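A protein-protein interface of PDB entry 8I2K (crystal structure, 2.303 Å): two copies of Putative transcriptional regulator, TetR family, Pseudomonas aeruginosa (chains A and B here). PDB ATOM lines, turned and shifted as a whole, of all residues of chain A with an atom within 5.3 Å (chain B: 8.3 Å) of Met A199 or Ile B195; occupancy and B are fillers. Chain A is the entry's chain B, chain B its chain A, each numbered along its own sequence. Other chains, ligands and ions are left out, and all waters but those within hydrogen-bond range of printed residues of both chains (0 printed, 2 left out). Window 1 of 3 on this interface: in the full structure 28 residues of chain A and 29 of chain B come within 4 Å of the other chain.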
ATOM      1  N   PHE A  93      23.484 -12.254   0.976  1.00  0.00           N
ATOM      2  CA  PHE A  93      24.840 -12.565   0.552  1.00  0.00           C
ATOM      3  C   PHE A  93      25.861 -11.715   1.295  1.00  0.00           C
ATOM      4  O   PHE A  93      26.926 -12.217   1.701  1.00  0.00           O
ATOM      5  CB  PHE A  93      24.964 -12.393  -0.967  1.00  0.00           C
ATOM      6  CG  PHE A  93      24.302 -13.481  -1.719  1.00  0.00           C
ATOM      7  CD1 PHE A  93      24.820 -14.780  -1.673  1.00  0.00           C
ATOM      8  CD2 PHE A  93      23.147 -13.228  -2.444  1.00  0.00           C
ATOM      9  CE1 PHE A  93      24.197 -15.791  -2.349  1.00  0.00           C
ATOM     10  CE2 PHE A  93      22.497 -14.252  -3.118  1.00  0.00           C
ATOM     11  CZ  PHE A  93      22.995 -15.530  -3.049  1.00  0.00           C
ATOM     12  N   LEU A 150      13.485 -15.302 -10.562  1.00  0.00           N
ATOM     13  CA  LEU A 150      14.320 -16.488 -10.563  1.00  0.00           C
ATOM     14  C   LEU A 150      13.739 -17.577 -11.457  1.00  0.00           C
ATOM     15  O   LEU A 150      12.522 -17.761 -11.555  1.00  0.00           O
ATOM     16  CB  LEU A 150      14.483 -17.060  -9.149  1.00  0.00           C
ATOM     17  CG  LEU A 150      15.363 -16.375  -8.117  1.00  0.00           C
ATOM     18  CD1 LEU A 150      15.424 -17.155  -6.775  1.00  0.00           C
ATOM     19  CD2 LEU A 150      16.739 -16.172  -8.653  1.00  0.00           C
ATOM     20  N   HIS A 158      18.329 -23.309  -6.217  1.00  0.00           N
ATOM     21  CA  HIS A 158      18.823 -21.988  -5.883  1.00  0.00           C
ATOM     22  C   HIS A 158      19.511 -21.983  -4.534  1.00  0.00           C
ATOM     23  O   HIS A 158      20.471 -21.228  -4.337  1.00  0.00           O
ATOM     24  CB  HIS A 158      17.686 -20.965  -5.869  1.00  0.00           C
ATOM     25  CG  HIS A 158      17.066 -20.717  -7.201  1.00  0.00           C
ATOM     26  ND1 HIS A 158      17.600 -19.843  -8.119  1.00  0.00           N
ATOM     27  CD2 HIS A 158      15.906 -21.157  -7.737  1.00  0.00           C
ATOM     28  CE1 HIS A 158      16.833 -19.810  -9.188  1.00  0.00           C
ATOM     29  NE2 HIS A 158      15.779 -20.572  -8.970  1.00  0.00           N
ATOM     30  N   ALA A 161      22.915 -23.591  -4.731  1.00  0.00           N
ATOM     31  CA  ALA A 161      23.798 -22.713  -5.484  1.00  0.00           C
ATOM     32  C   ALA A 161      24.265 -21.534  -4.634  1.00  0.00           C
ATOM     33  O   ALA A 161      25.433 -21.141  -4.689  1.00  0.00           O
ATOM     34  CB  ALA A 161      23.087 -22.220  -6.745  1.00  0.00           C
ATOM     35  N   ALA A 162      23.366 -20.943  -3.855  1.00  0.00           N
ATOM     36  CA  ALA A 162      23.778 -19.906  -2.920  1.00  0.00           C
ATOM     37  C   ALA A 162      24.770 -20.455  -1.891  1.00  0.00           C
ATOM     38  O   ALA A 162      25.728 -19.774  -1.532  1.00  0.00           O
ATOM     39  CB  ALA A 162      22.537 -19.316  -2.247  1.00  0.00           C
ATOM     40  N   LEU A 165      28.296 -20.809  -3.721  1.00  0.00           N
ATOM     41  CA  LEU A 165      28.906 -19.492  -3.889  1.00  0.00           C
ATOM     42  C   LEU A 165      29.499 -18.979  -2.579  1.00  0.00           C
ATOM     43  O   LEU A 165      30.670 -18.593  -2.527  1.00  0.00           O
ATOM     44  CB  LEU A 165      27.878 -18.508  -4.448  1.00  0.00           C
ATOM     45  CG  LEU A 165      28.419 -17.110  -4.717  1.00  0.00           C
ATOM     46  CD1 LEU A 165      29.535 -17.211  -5.766  1.00  0.00           C
ATOM     47  CD2 LEU A 165      27.370 -16.184  -5.220  1.00  0.00           C
ATOM     48  N   ASP A 194      26.715  -8.843  -6.277  1.00  0.00           N
ATOM     49  CA  ASP A 194      25.920  -8.779  -7.493  1.00  0.00           C
ATOM     50  C   ASP A 194      25.716 -10.182  -8.066  1.00  0.00           C
ATOM     51  O   ASP A 194      24.612 -10.538  -8.492  1.00  0.00           O
ATOM     52  CB  ASP A 194      26.569  -7.880  -8.548  1.00  0.00           C
ATOM     53  CG  ASP A 194      26.548  -6.375  -8.178  1.00  0.00           C
ATOM     54  OD1 ASP A 194      25.843  -5.980  -7.219  1.00  0.00           O
ATOM     55  OD2 ASP A 194      27.265  -5.577  -8.863  1.00  0.00           O
ATOM     56  N   ILE A 195      26.775 -10.993  -8.078  1.00  0.00           N
ATOM     57  CA  ILE A 195      26.687 -12.315  -8.687  1.00  0.00           C
ATOM     58  C   ILE A 195      25.679 -13.191  -7.944  1.00  0.00           C
ATOM     59  O   ILE A 195      24.889 -13.914  -8.558  1.00  0.00           O
ATOM     60  CB  ILE A 195      28.084 -12.960  -8.736  1.00  0.00           C
ATOM     61  CG1 ILE A 195      28.913 -12.260  -9.827  1.00  0.00           C
ATOM     62  CG2 ILE A 195      27.953 -14.446  -8.925  1.00  0.00           C
ATOM     63  CD1 ILE A 195      30.339 -12.773  -9.894  1.00  0.00           C
ATOM     64  N   GLY A 196      25.700 -13.154  -6.617  1.00  0.00           N
ATOM     65  CA  GLY A 196      24.732 -13.929  -5.858  1.00  0.00           C
ATOM     66  C   GLY A 196      23.303 -13.507  -6.120  1.00  0.00           C
ATOM     67  O   GLY A 196      22.430 -14.352  -6.300  1.00  0.00           O
ATOM     68  N   VAL A 197      23.047 -12.196  -6.165  1.00  0.00           N
ATOM     69  CA  VAL A 197      21.718 -11.698  -6.485  1.00  0.00           C
ATOM     70  C   VAL A 197      21.307 -12.145  -7.878  1.00  0.00           C
ATOM     71  O   VAL A 197      20.136 -12.430  -8.134  1.00  0.00           O
ATOM     72  CB  VAL A 197      21.685 -10.163  -6.369  1.00  0.00           C
ATOM     73  CG1 VAL A 197      20.332  -9.621  -6.824  1.00  0.00           C
ATOM     74  CG2 VAL A 197      21.995  -9.716  -4.954  1.00  0.00           C
ATOM     75  N   ARG A 198      22.260 -12.198  -8.809  1.00  0.00           N
ATOM     76  CA  ARG A 198      21.935 -12.472 -10.202  1.00  0.00           C
ATOM     77  C   ARG A 198      21.956 -13.952 -10.514  1.00  0.00           C
ATOM     78  O   ARG A 198      21.418 -14.356 -11.546  1.00  0.00           O
ATOM     79  CB  ARG A 198      22.882 -11.696 -11.125  1.00  0.00           C
ATOM     80  CG  ARG A 198      22.446 -10.250 -11.359  1.00  0.00           C
ATOM     81  CD  ARG A 198      23.548  -9.220 -11.216  1.00  0.00           C
ATOM     82  NE  ARG A 198      24.339  -9.050 -12.446  1.00  0.00           N
ATOM     83  CZ  ARG A 198      25.045  -7.956 -12.771  1.00  0.00           C
ATOM     84  NH1 ARG A 198      25.067  -6.889 -11.970  1.00  0.00           N
ATOM     85  NH2 ARG A 198      25.744  -7.935 -13.908  1.00  0.00           N
ATOM     86  N   MET A 199      22.456 -14.773  -9.596  1.00  0.00           N
ATOM     87  CA  MET A 199      22.497 -16.212  -9.818  1.00  0.00           C
ATOM     88  C   MET A 199      21.106 -16.771 -10.094  1.00  0.00           C
ATOM     89  O   MET A 199      20.169 -16.522  -9.332  1.00  0.00           O
ATOM     90  CB  MET A 199      23.082 -16.907  -8.592  1.00  0.00           C
ATOM     91  CG  MET A 199      24.477 -17.325  -8.719  1.00  0.00           C
ATOM     92  SD  MET A 199      25.034 -18.579  -7.528  1.00  0.00           S
ATOM     93  CE  MET A 199      24.294 -18.082  -5.971  1.00  0.00           C
ATOM     94  N   GLY A 200      20.982 -17.546 -11.168  1.00  0.00           N
ATOM     95  CA  GLY A 200      19.732 -18.217 -11.485  1.00  0.00           C
ATOM     96  C   GLY A 200      18.575 -17.324 -11.904  1.00  0.00           C
ATOM     97  O   GLY A 200      17.420 -17.770 -11.895  1.00  0.00           O
ATOM     98  N   ASN A 201      18.840 -16.076 -12.266  1.00  0.00           N
ATOM     99  CA  ASN A 201      17.774 -15.201 -12.722  1.00  0.00           C
ATOM    100  C   ASN A 201      17.184 -15.720 -14.033  1.00  0.00           C
ATOM    101  O   ASN A 201      17.878 -16.323 -14.854  1.00  0.00           O
ATOM    102  CB  ASN A 201      18.316 -13.791 -12.865  1.00  0.00           C
ATOM    103  CG  ASN A 201      18.638 -13.167 -11.522  1.00  0.00           C
ATOM    104  OD1 ASN A 201      18.764 -13.870 -10.510  1.00  0.00           O
ATOM    105  ND2 ASN A 201      18.743 -11.854 -11.491  1.00  0.00           N
ATOM    106  N   SER B  89      33.414 -21.406 -22.240  1.00  0.00           N
ATOM    107  CA  SER B  89      33.084 -21.155 -20.842  1.00  0.00           C
ATOM    108  C   SER B  89      32.302 -22.322 -20.241  1.00  0.00           C
ATOM    109  O   SER B  89      32.692 -22.875 -19.208  1.00  0.00           O
ATOM    110  CB  SER B  89      32.298 -19.861 -20.728  1.00  0.00           C
ATOM    111  OG  SER B  89      32.057 -19.522 -19.377  1.00  0.00           O
ATOM    112  N   ARG B  90      31.276 -22.799 -20.942  1.00  0.00           N
ATOM    113  CA  ARG B  90      30.538 -23.951 -20.426  1.00  0.00           C
ATOM    114  C   ARG B  90      31.444 -25.174 -20.320  1.00  0.00           C
ATOM    115  O   ARG B  90      31.451 -25.878 -19.304  1.00  0.00           O
ATOM    116  CB  ARG B  90      29.324 -24.233 -21.320  1.00  0.00           C
ATOM    117  CG  ARG B  90      28.399 -25.353 -20.786  1.00  0.00           C
ATOM    118  CD  ARG B  90      27.036 -25.444 -21.560  1.00  0.00           C
ATOM    119  NE  ARG B  90      26.467 -24.109 -21.708  1.00  0.00           N
ATOM    120  CZ  ARG B  90      25.577 -23.588 -20.863  1.00  0.00           C
ATOM    121  NH1 ARG B  90      25.126 -24.316 -19.835  1.00  0.00           N
ATOM    122  NH2 ARG B  90      25.135 -22.342 -21.046  1.00  0.00           N
ATOM    123  N   PHE B  93      33.649 -24.889 -17.097  1.00  0.00           N
ATOM    124  CA  PHE B  93      32.977 -25.267 -15.847  1.00  0.00           C
ATOM    125  C   PHE B  93      32.681 -26.763 -15.793  1.00  0.00           C
ATOM    126  O   PHE B  93      32.866 -27.391 -14.746  1.00  0.00           O
ATOM    127  CB  PHE B  93      31.689 -24.468 -15.642  1.00  0.00           C
ATOM    128  CG  PHE B  93      31.957 -23.057 -15.287  1.00  0.00           C
ATOM    129  CD1 PHE B  93      32.480 -22.726 -14.030  1.00  0.00           C
ATOM    130  CD2 PHE B  93      31.772 -22.061 -16.216  1.00  0.00           C
ATOM    131  CE1 PHE B  93      32.790 -21.420 -13.727  1.00  0.00           C
ATOM    132  CE2 PHE B  93      32.072 -20.762 -15.911  1.00  0.00           C
ATOM    133  CZ  PHE B  93      32.586 -20.435 -14.691  1.00  0.00           C
ATOM    134  N   MET B  97      34.051 -29.216 -12.830  1.00  0.00           N
ATOM    135  CA  MET B  97      33.124 -29.800 -11.871  1.00  0.00           C
ATOM    136  C   MET B  97      32.820 -31.273 -12.151  1.00  0.00           C
ATOM    137  O   MET B  97      32.143 -31.909 -11.359  1.00  0.00           O
ATOM    138  CB  MET B  97      31.820 -28.984 -11.853  1.00  0.00           C
ATOM    139  CG  MET B  97      31.953 -27.661 -11.142  1.00  0.00           C
ATOM    140  SD  MET B  97      30.452 -26.680 -11.413  1.00  0.00           S
ATOM    141  CE  MET B  97      31.075 -25.044 -11.762  1.00  0.00           C
ATOM    142  N   ARG B 144      35.690 -12.240 -23.482  1.00  0.00           N
ATOM    143  CA  ARG B 144      34.258 -12.145 -23.246  1.00  0.00           C
ATOM    144  C   ARG B 144      33.873 -10.757 -22.759  1.00  0.00           C
ATOM    145  O   ARG B 144      32.763 -10.277 -23.054  1.00  0.00           O
ATOM    146  CB  ARG B 144      33.841 -13.235 -22.277  1.00  0.00           C
ATOM    147  CG  ARG B 144      33.987 -14.589 -22.924  1.00  0.00           C
ATOM    148  CD  ARG B 144      33.668 -15.675 -21.922  1.00  0.00           C
ATOM    149  NE  ARG B 144      32.215 -15.781 -21.711  1.00  0.00           N
ATOM    150  CZ  ARG B 144      31.623 -16.076 -20.558  1.00  0.00           C
ATOM    151  NH1 ARG B 144      32.344 -16.300 -19.456  1.00  0.00           N
ATOM    152  NH2 ARG B 144      30.302 -16.183 -20.524  1.00  0.00           N
ATOM    153  N   ALA B 161      35.674 -15.256  -8.989  1.00  0.00           N
ATOM    154  CA  ALA B 161      34.305 -15.756  -9.008  1.00  0.00           C
ATOM    155  C   ALA B 161      34.247 -17.197  -9.483  1.00  0.00           C
ATOM    156  O   ALA B 161      33.598 -18.053  -8.857  1.00  0.00           O
ATOM    157  CB  ALA B 161      33.421 -14.890  -9.912  1.00  0.00           C
ATOM    158  N   LEU B 165      33.058 -20.468  -7.309  1.00  0.00           N
ATOM    159  CA  LEU B 165      31.902 -21.274  -7.670  1.00  0.00           C
ATOM    160  C   LEU B 165      32.274 -22.741  -7.764  1.00  0.00           C
ATOM    161  O   LEU B 165      31.581 -23.607  -7.221  1.00  0.00           O
ATOM    162  CB  LEU B 165      31.316 -20.770  -8.982  1.00  0.00           C
ATOM    163  CG  LEU B 165      30.036 -21.517  -9.369  1.00  0.00           C
ATOM    164  CD1 LEU B 165      28.864 -21.194  -8.461  1.00  0.00           C
ATOM    165  CD2 LEU B 165      29.643 -21.224 -10.796  1.00  0.00           C
ATOM    166  N   PHE B 188      20.501 -30.509 -11.645  1.00  0.00           N
ATOM    167  CA  PHE B 188      21.187 -29.484 -10.885  1.00  0.00           C
ATOM    168  C   PHE B 188      22.506 -29.121 -11.547  1.00  0.00           C
ATOM    169  O   PHE B 188      22.844 -27.937 -11.688  1.00  0.00           O
ATOM    170  CB  PHE B 188      21.451 -29.931  -9.464  1.00  0.00           C
ATOM    171  CG  PHE B 188      22.148 -28.881  -8.667  1.00  0.00           C
ATOM    172  CD1 PHE B 188      21.498 -27.705  -8.338  1.00  0.00           C
ATOM    173  CD2 PHE B 188      23.470 -29.029  -8.315  1.00  0.00           C
ATOM    174  CE1 PHE B 188      22.157 -26.721  -7.639  1.00  0.00           C
ATOM    175  CE2 PHE B 188      24.125 -28.041  -7.615  1.00  0.00           C
ATOM    176  CZ  PHE B 188      23.479 -26.899  -7.284  1.00  0.00           C
ATOM    177  N   PHE B 189      23.252 -30.136 -11.965  1.00  0.00           N
ATOM    178  CA  PHE B 189      24.536 -29.922 -12.619  1.00  0.00           C
ATOM    179  C   PHE B 189      24.424 -28.956 -13.792  1.00  0.00           C
ATOM    180  O   PHE B 189      25.200 -27.995 -13.896  1.00  0.00           O
ATOM    181  CB  PHE B 189      25.090 -31.263 -13.075  1.00  0.00           C
ATOM    182  CG  PHE B 189      26.470 -31.186 -13.612  1.00  0.00           C
ATOM    183  CD1 PHE B 189      27.559 -31.262 -12.761  1.00  0.00           C
ATOM    184  CD2 PHE B 189      26.682 -31.013 -14.971  1.00  0.00           C
ATOM    185  CE1 PHE B 189      28.847 -31.190 -13.258  1.00  0.00           C
ATOM    186  CE2 PHE B 189      27.958 -30.937 -15.472  1.00  0.00           C
ATOM    187  CZ  PHE B 189      29.050 -31.035 -14.615  1.00  0.00           C
ATOM    188  N   HIS B 190      23.455 -29.187 -14.681  1.00  0.00           N
ATOM    189  CA  HIS B 190      23.267 -28.285 -15.811  1.00  0.00           C
ATOM    190  C   HIS B 190      22.833 -26.895 -15.354  1.00  0.00           C
ATOM    191  O   HIS B 190      23.255 -25.888 -15.938  1.00  0.00           O
ATOM    192  CB  HIS B 190      22.297 -28.926 -16.803  1.00  0.00           C
ATOM    193  CG  HIS B 190      22.927 -30.062 -17.566  1.00  0.00           C
ATOM    194  ND1 HIS B 190      24.135 -29.936 -18.226  1.00  0.00           N
ATOM    195  CD2 HIS B 190      22.552 -31.354 -17.727  1.00  0.00           C
ATOM    196  CE1 HIS B 190      24.461 -31.090 -18.778  1.00  0.00           C
ATOM    197  NE2 HIS B 190      23.517 -31.970 -18.487  1.00  0.00           N
ATOM    198  N   PHE B 191      22.011 -26.804 -14.308  1.00  0.00           N
ATOM    199  CA  PHE B 191      21.710 -25.499 -13.726  1.00  0.00           C
ATOM    200  C   PHE B 191      22.998 -24.801 -13.259  1.00  0.00           C
ATOM    201  O   PHE B 191      23.193 -23.601 -13.489  1.00  0.00           O
ATOM    202  CB  PHE B 191      20.696 -25.713 -12.594  1.00  0.00           C
ATOM    203  CG  PHE B 191      20.378 -24.486 -11.815  1.00  0.00           C
ATOM    204  CD1 PHE B 191      19.554 -23.518 -12.337  1.00  0.00           C
ATOM    205  CD2 PHE B 191      20.857 -24.327 -10.526  1.00  0.00           C
ATOM    206  CE1 PHE B 191      19.239 -22.368 -11.607  1.00  0.00           C
ATOM    207  CE2 PHE B 191      20.538 -23.177  -9.782  1.00  0.00           C
ATOM    208  CZ  PHE B 191      19.747 -22.194 -10.336  1.00  0.00           C
ATOM    209  N   LEU B 192      23.919 -25.558 -12.673  1.00  0.00           N
ATOM    210  CA  LEU B 192      25.169 -24.996 -12.177  1.00  0.00           C
ATOM    211  C   LEU B 192      26.049 -24.473 -13.309  1.00  0.00           C
ATOM    212  O   LEU B 192      26.704 -23.436 -13.165  1.00  0.00           O
ATOM    213  CB  LEU B 192      25.906 -26.077 -11.410  1.00  0.00           C
ATOM    214  CG  LEU B 192      26.240 -25.962  -9.933  1.00  0.00           C
ATOM    215  CD1 LEU B 192      27.261 -27.061  -9.587  1.00  0.00           C
ATOM    216  CD2 LEU B 192      26.777 -24.619  -9.669  1.00  0.00           C
ATOM    217  N   MET B 193      26.107 -25.221 -14.409  1.00  0.00           N
ATOM    218  CA  MET B 193      26.788 -24.787 -15.613  1.00  0.00           C
ATOM    219  C   MET B 193      26.210 -23.477 -16.113  1.00  0.00           C
ATOM    220  O   MET B 193      26.953 -22.563 -16.482  1.00  0.00           O
ATOM    221  CB  MET B 193      26.655 -25.861 -16.693  1.00  0.00           C
ATOM    222  CG  MET B 193      27.372 -27.183 -16.427  1.00  0.00           C
ATOM    223  SD  MET B 193      29.031 -27.081 -15.799  1.00  0.00           S
ATOM    224  CE  MET B 193      28.693 -26.858 -14.056  1.00  0.00           C
ATOM    225  N   ASP B 194      24.880 -23.386 -16.191  1.00  0.00           N
ATOM    226  CA  ASP B 194      24.272 -22.134 -16.626  1.00  0.00           C
ATOM    227  C   ASP B 194      24.720 -21.006 -15.712  1.00  0.00           C
ATOM    228  O   ASP B 194      25.117 -19.935 -16.180  1.00  0.00           O
ATOM    229  CB  ASP B 194      22.740 -22.214 -16.652  1.00  0.00           C
ATOM    230  CG  ASP B 194      22.205 -23.116 -17.764  1.00  0.00           C
ATOM    231  OD1 ASP B 194      22.999 -23.547 -18.612  1.00  0.00           O
ATOM    232  OD2 ASP B 194      20.984 -23.419 -17.779  1.00  0.00           O
ATOM    233  N   ILE B 195      24.670 -21.234 -14.392  1.00  0.00           N
ATOM    234  CA  ILE B 195      25.122 -20.196 -13.474  1.00  0.00           C
ATOM    235  C   ILE B 195      26.542 -19.749 -13.831  1.00  0.00           C
ATOM    236  O   ILE B 195      26.821 -18.550 -13.914  1.00  0.00           O
ATOM    237  CB  ILE B 195      25.001 -20.672 -12.015  1.00  0.00           C
ATOM    238  CG1 ILE B 195      23.528 -20.525 -11.610  1.00  0.00           C
ATOM    239  CG2 ILE B 195      25.930 -19.866 -11.095  1.00  0.00           C
ATOM    240  CD1 ILE B 195      23.202 -21.162 -10.320  1.00  0.00           C
ATOM    241  N   GLY B 196      27.440 -20.699 -14.098  1.00  0.00           N
ATOM    242  CA  GLY B 196      28.837 -20.346 -14.330  1.00  0.00           C
ATOM    243  C   GLY B 196      29.043 -19.519 -15.597  1.00  0.00           C
ATOM    244  O   GLY B 196      29.678 -18.459 -15.573  1.00  0.00           O
ATOM    245  N   VAL B 197      28.465 -19.976 -16.705  1.00  0.00           N
ATOM    246  CA  VAL B 197      28.480 -19.219 -17.955  1.00  0.00           C
ATOM    247  C   VAL B 197      27.886 -17.823 -17.802  1.00  0.00           C
ATOM    248  O   VAL B 197      28.313 -16.871 -18.467  1.00  0.00           O
ATOM    249  CB  VAL B 197      27.744 -20.014 -19.032  1.00  0.00           C
ATOM    250  CG1 VAL B 197      27.556 -19.159 -20.255  1.00  0.00           C
ATOM    251  CG2 VAL B 197      28.537 -21.270 -19.310  1.00  0.00           C
ATOM    252  N   ARG B 198      26.888 -17.680 -16.954  1.00  0.00           N
ATOM    253  CA  ARG B 198      26.138 -16.442 -16.856  1.00  0.00           C
ATOM    254  C   ARG B 198      26.696 -15.521 -15.790  1.00  0.00           C
ATOM    255  O   ARG B 198      26.345 -14.338 -15.745  1.00  0.00           O
ATOM    256  CB  ARG B 198      24.656 -16.783 -16.595  1.00  0.00           C
ATOM    257  CG  ARG B 198      23.872 -16.920 -17.934  1.00  0.00           C
ATOM    258  CD  ARG B 198      22.820 -18.002 -17.985  1.00  0.00           C
ATOM    259  NE  ARG B 198      21.527 -17.482 -17.565  1.00  0.00           N
ATOM    260  CZ  ARG B 198      20.376 -18.139 -17.677  1.00  0.00           C
ATOM    261  NH1 ARG B 198      20.339 -19.356 -18.216  1.00  0.00           N
ATOM    262  NH2 ARG B 198      19.259 -17.572 -17.250  1.00  0.00           N
ATOM    263  N   MET B 199      27.586 -16.029 -14.970  1.00  0.00           N
ATOM    264  CA  MET B 199      28.119 -15.261 -13.858  1.00  0.00           C
ATOM    265  C   MET B 199      28.840 -14.029 -14.366  1.00  0.00           C
ATOM    266  O   MET B 199      29.634 -14.106 -15.310  1.00  0.00           O
ATOM    267  CB  MET B 199      29.084 -16.139 -13.070  1.00  0.00           C
ATOM    268  CG  MET B 199      29.288 -15.735 -11.665  1.00  0.00           C
ATOM    269  SD  MET B 199      30.049 -17.041 -10.671  1.00  0.00           S
ATOM    270  CE  MET B 199      31.370 -17.669 -11.674  1.00  0.00           C
ATOM    271  N   GLY B 200      28.562 -12.896 -13.736  1.00  0.00           N
ATOM    272  CA  GLY B 200      29.241 -11.674 -14.089  1.00  0.00           C
ATOM    273  C   GLY B 200      28.961 -11.179 -15.486  1.00  0.00           C
ATOM    274  O   GLY B 200      29.744 -10.392 -16.013  1.00  0.00           O
ATOM    275  N   ASN B 201      27.867 -11.630 -16.100  1.00  0.00           N
ATOM    276  CA  ASN B 201      27.450 -11.137 -17.400  1.00  0.00           C
ATOM    277  C   ASN B 201      27.063  -9.669 -17.294  1.00  0.00           C
ATOM    278  O   ASN B 201      26.516  -9.232 -16.287  1.00  0.00           O
ATOM    279  CB  ASN B 201      26.274 -11.970 -17.923  1.00  0.00           C
ATOM    280  CG  ASN B 201      26.696 -13.342 -18.481  1.00  0.00           C
ATOM    281  OD1 ASN B 201      25.942 -13.967 -19.230  1.00  0.00           O
ATOM    282  ND2 ASN B 201      27.884 -13.829 -18.093  1.00  0.00           N
ATOM    283  N   ARG B 203      24.861  -6.516 -17.605  1.00  0.00           N
ATOM    284  CA  ARG B 203      23.406  -6.294 -17.584  1.00  0.00           C
ATOM    285  C   ARG B 203      22.908  -5.595 -18.846  1.00  0.00           C
ATOM    286  O   ARG B 203      23.025  -4.369 -18.947  1.00  0.00           O
ATOM    287  CB  ARG B 203      22.984  -5.430 -16.382  1.00  0.00           C
ATOM    288  CG  ARG B 203      23.087  -6.079 -14.996  1.00  0.00           C
ATOM    289  CD  ARG B 203      22.276  -7.377 -14.899  1.00  0.00           C
ATOM    290  NE  ARG B 203      21.079  -7.245 -14.057  1.00  0.00           N
ATOM    291  CZ  ARG B 203      20.311  -8.262 -13.658  1.00  0.00           C
ATOM    292  NH1 ARG B 203      20.608  -9.515 -14.022  1.00  0.00           N
ATOM    293  NH2 ARG B 203      19.238  -8.021 -12.900  1.00  0.00           N
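The guanidinium group (NH2) of Arg B198 is in hydrogen-bond range of the backbone carbonyl oxygen (O) of Asn A201, 3.0 Å away.
The backbone carbonyl oxygen (O) of Asn B201 is in hydrogen-bond range of the guanidinium group (NH2) of Arg A198 (2.8 Å).
O of Val B197 lies within hydrogen-bond range of ND2 of Asn B201 (3.1 Å).
The backbone carbonyl oxygen of Arg B198 is in hydrogen-bond range of the side-chain amide nitrogen of Asn B201 (2.9 Å).
O of Met B199 is in hydrogen-bond range of ND2 of Asn B201 (3.3 Å).
The backbone carbonyl oxygen of Val A197 lies close to the side-chain amide oxygen of Asn A201.
The backbone carbonyl oxygen of Arg A198 sits close to the side-chain amide oxygen of Asn A201.
OD1 of Asn A201 sits close to O of Met A199 (3.2 Å).
His A158 touches Phe B191 (ND1 to CZ, 3.9 Å).
Ala A161 touches Ile B195.
Ile A195 touches Ala B161.
Ile A195 touches Met B199 (CG2 to CG, 3.3 Å).
N of Gly B200 touches CG1 of Ile A195, 3.98 Å away.
Arg A198 touches Arg B203 (CG to NH1, 3.3 Å).
CG2 of Ile B195 touches CG of Met A199, 3.8 Å away.
Gly A200 touches Ile B195 (N to CG1, 3.9 Å).
ND2 of Asn A201 touches NH1 of Arg B203, at 3.9 Å.
Of the printed residues of chain B, His A158 touches Phe B191.
Printed residues of chain B within 4 Å of Ile A195: Ala B161, Met B199 and Gly B200.
Val A197 touches none of the printed residues of chain B.
Printed residues of chain B within 4 Å of Arg A198: Asn B201 (2.8 Å) and Arg B203 (3.3 Å).
Of chain B, only Ile B195 comes within 4 Å of Gly A200.
Printed residues of chain B within 4 Å of Asn A201: Arg B198 and Arg B203.
Leu B165 touches none of the printed residues of chain A.
Ile B195 touches just these residues of chain A: Ala A161 (3.7 Å), Met A199 (3.8 Å) and Gly A200 (3.9 Å).
Of the printed residues of chain A, Gly B200 touches Ile A195.
The nearest residue of chain B that does not touch Met A199 is Leu B165 (4.7 Å).
The nearest printed residue of chain A that does not touch Ile B195 is His A158 (6.2 Å).
Of the 14 printed residues of chain A, 7 touch a printed residue of chain B.
Hydrophobic or aromatic side chains of chain A within 4 Å of the printed part of chain B: His A158, Ala A161, Ile A195 and Met A199.
Among the printed residues, no Asp or Glu carboxylate lies within 4 Å of a Lys or Arg side-chain nitrogen of the other chain.
Ala A161 touches Ile B195, and with the chains exchanged Ile A195 touches Ala B161.
Ile A195 touches Met B199, and with the chains exchanged Met A199 touches Ile B195.
Ile A195 touches Gly B200, and with the chains exchanged Gly A200 touches Ile B195.
Arg A198 touches Asn B201, and with the chains exchanged Asn A201 touches Arg B198.
11 positions are printed for both chains.
Of the 11 pairs that touch across the chains among the printed residues, 8 have their exchanged pair printed and touching as well.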
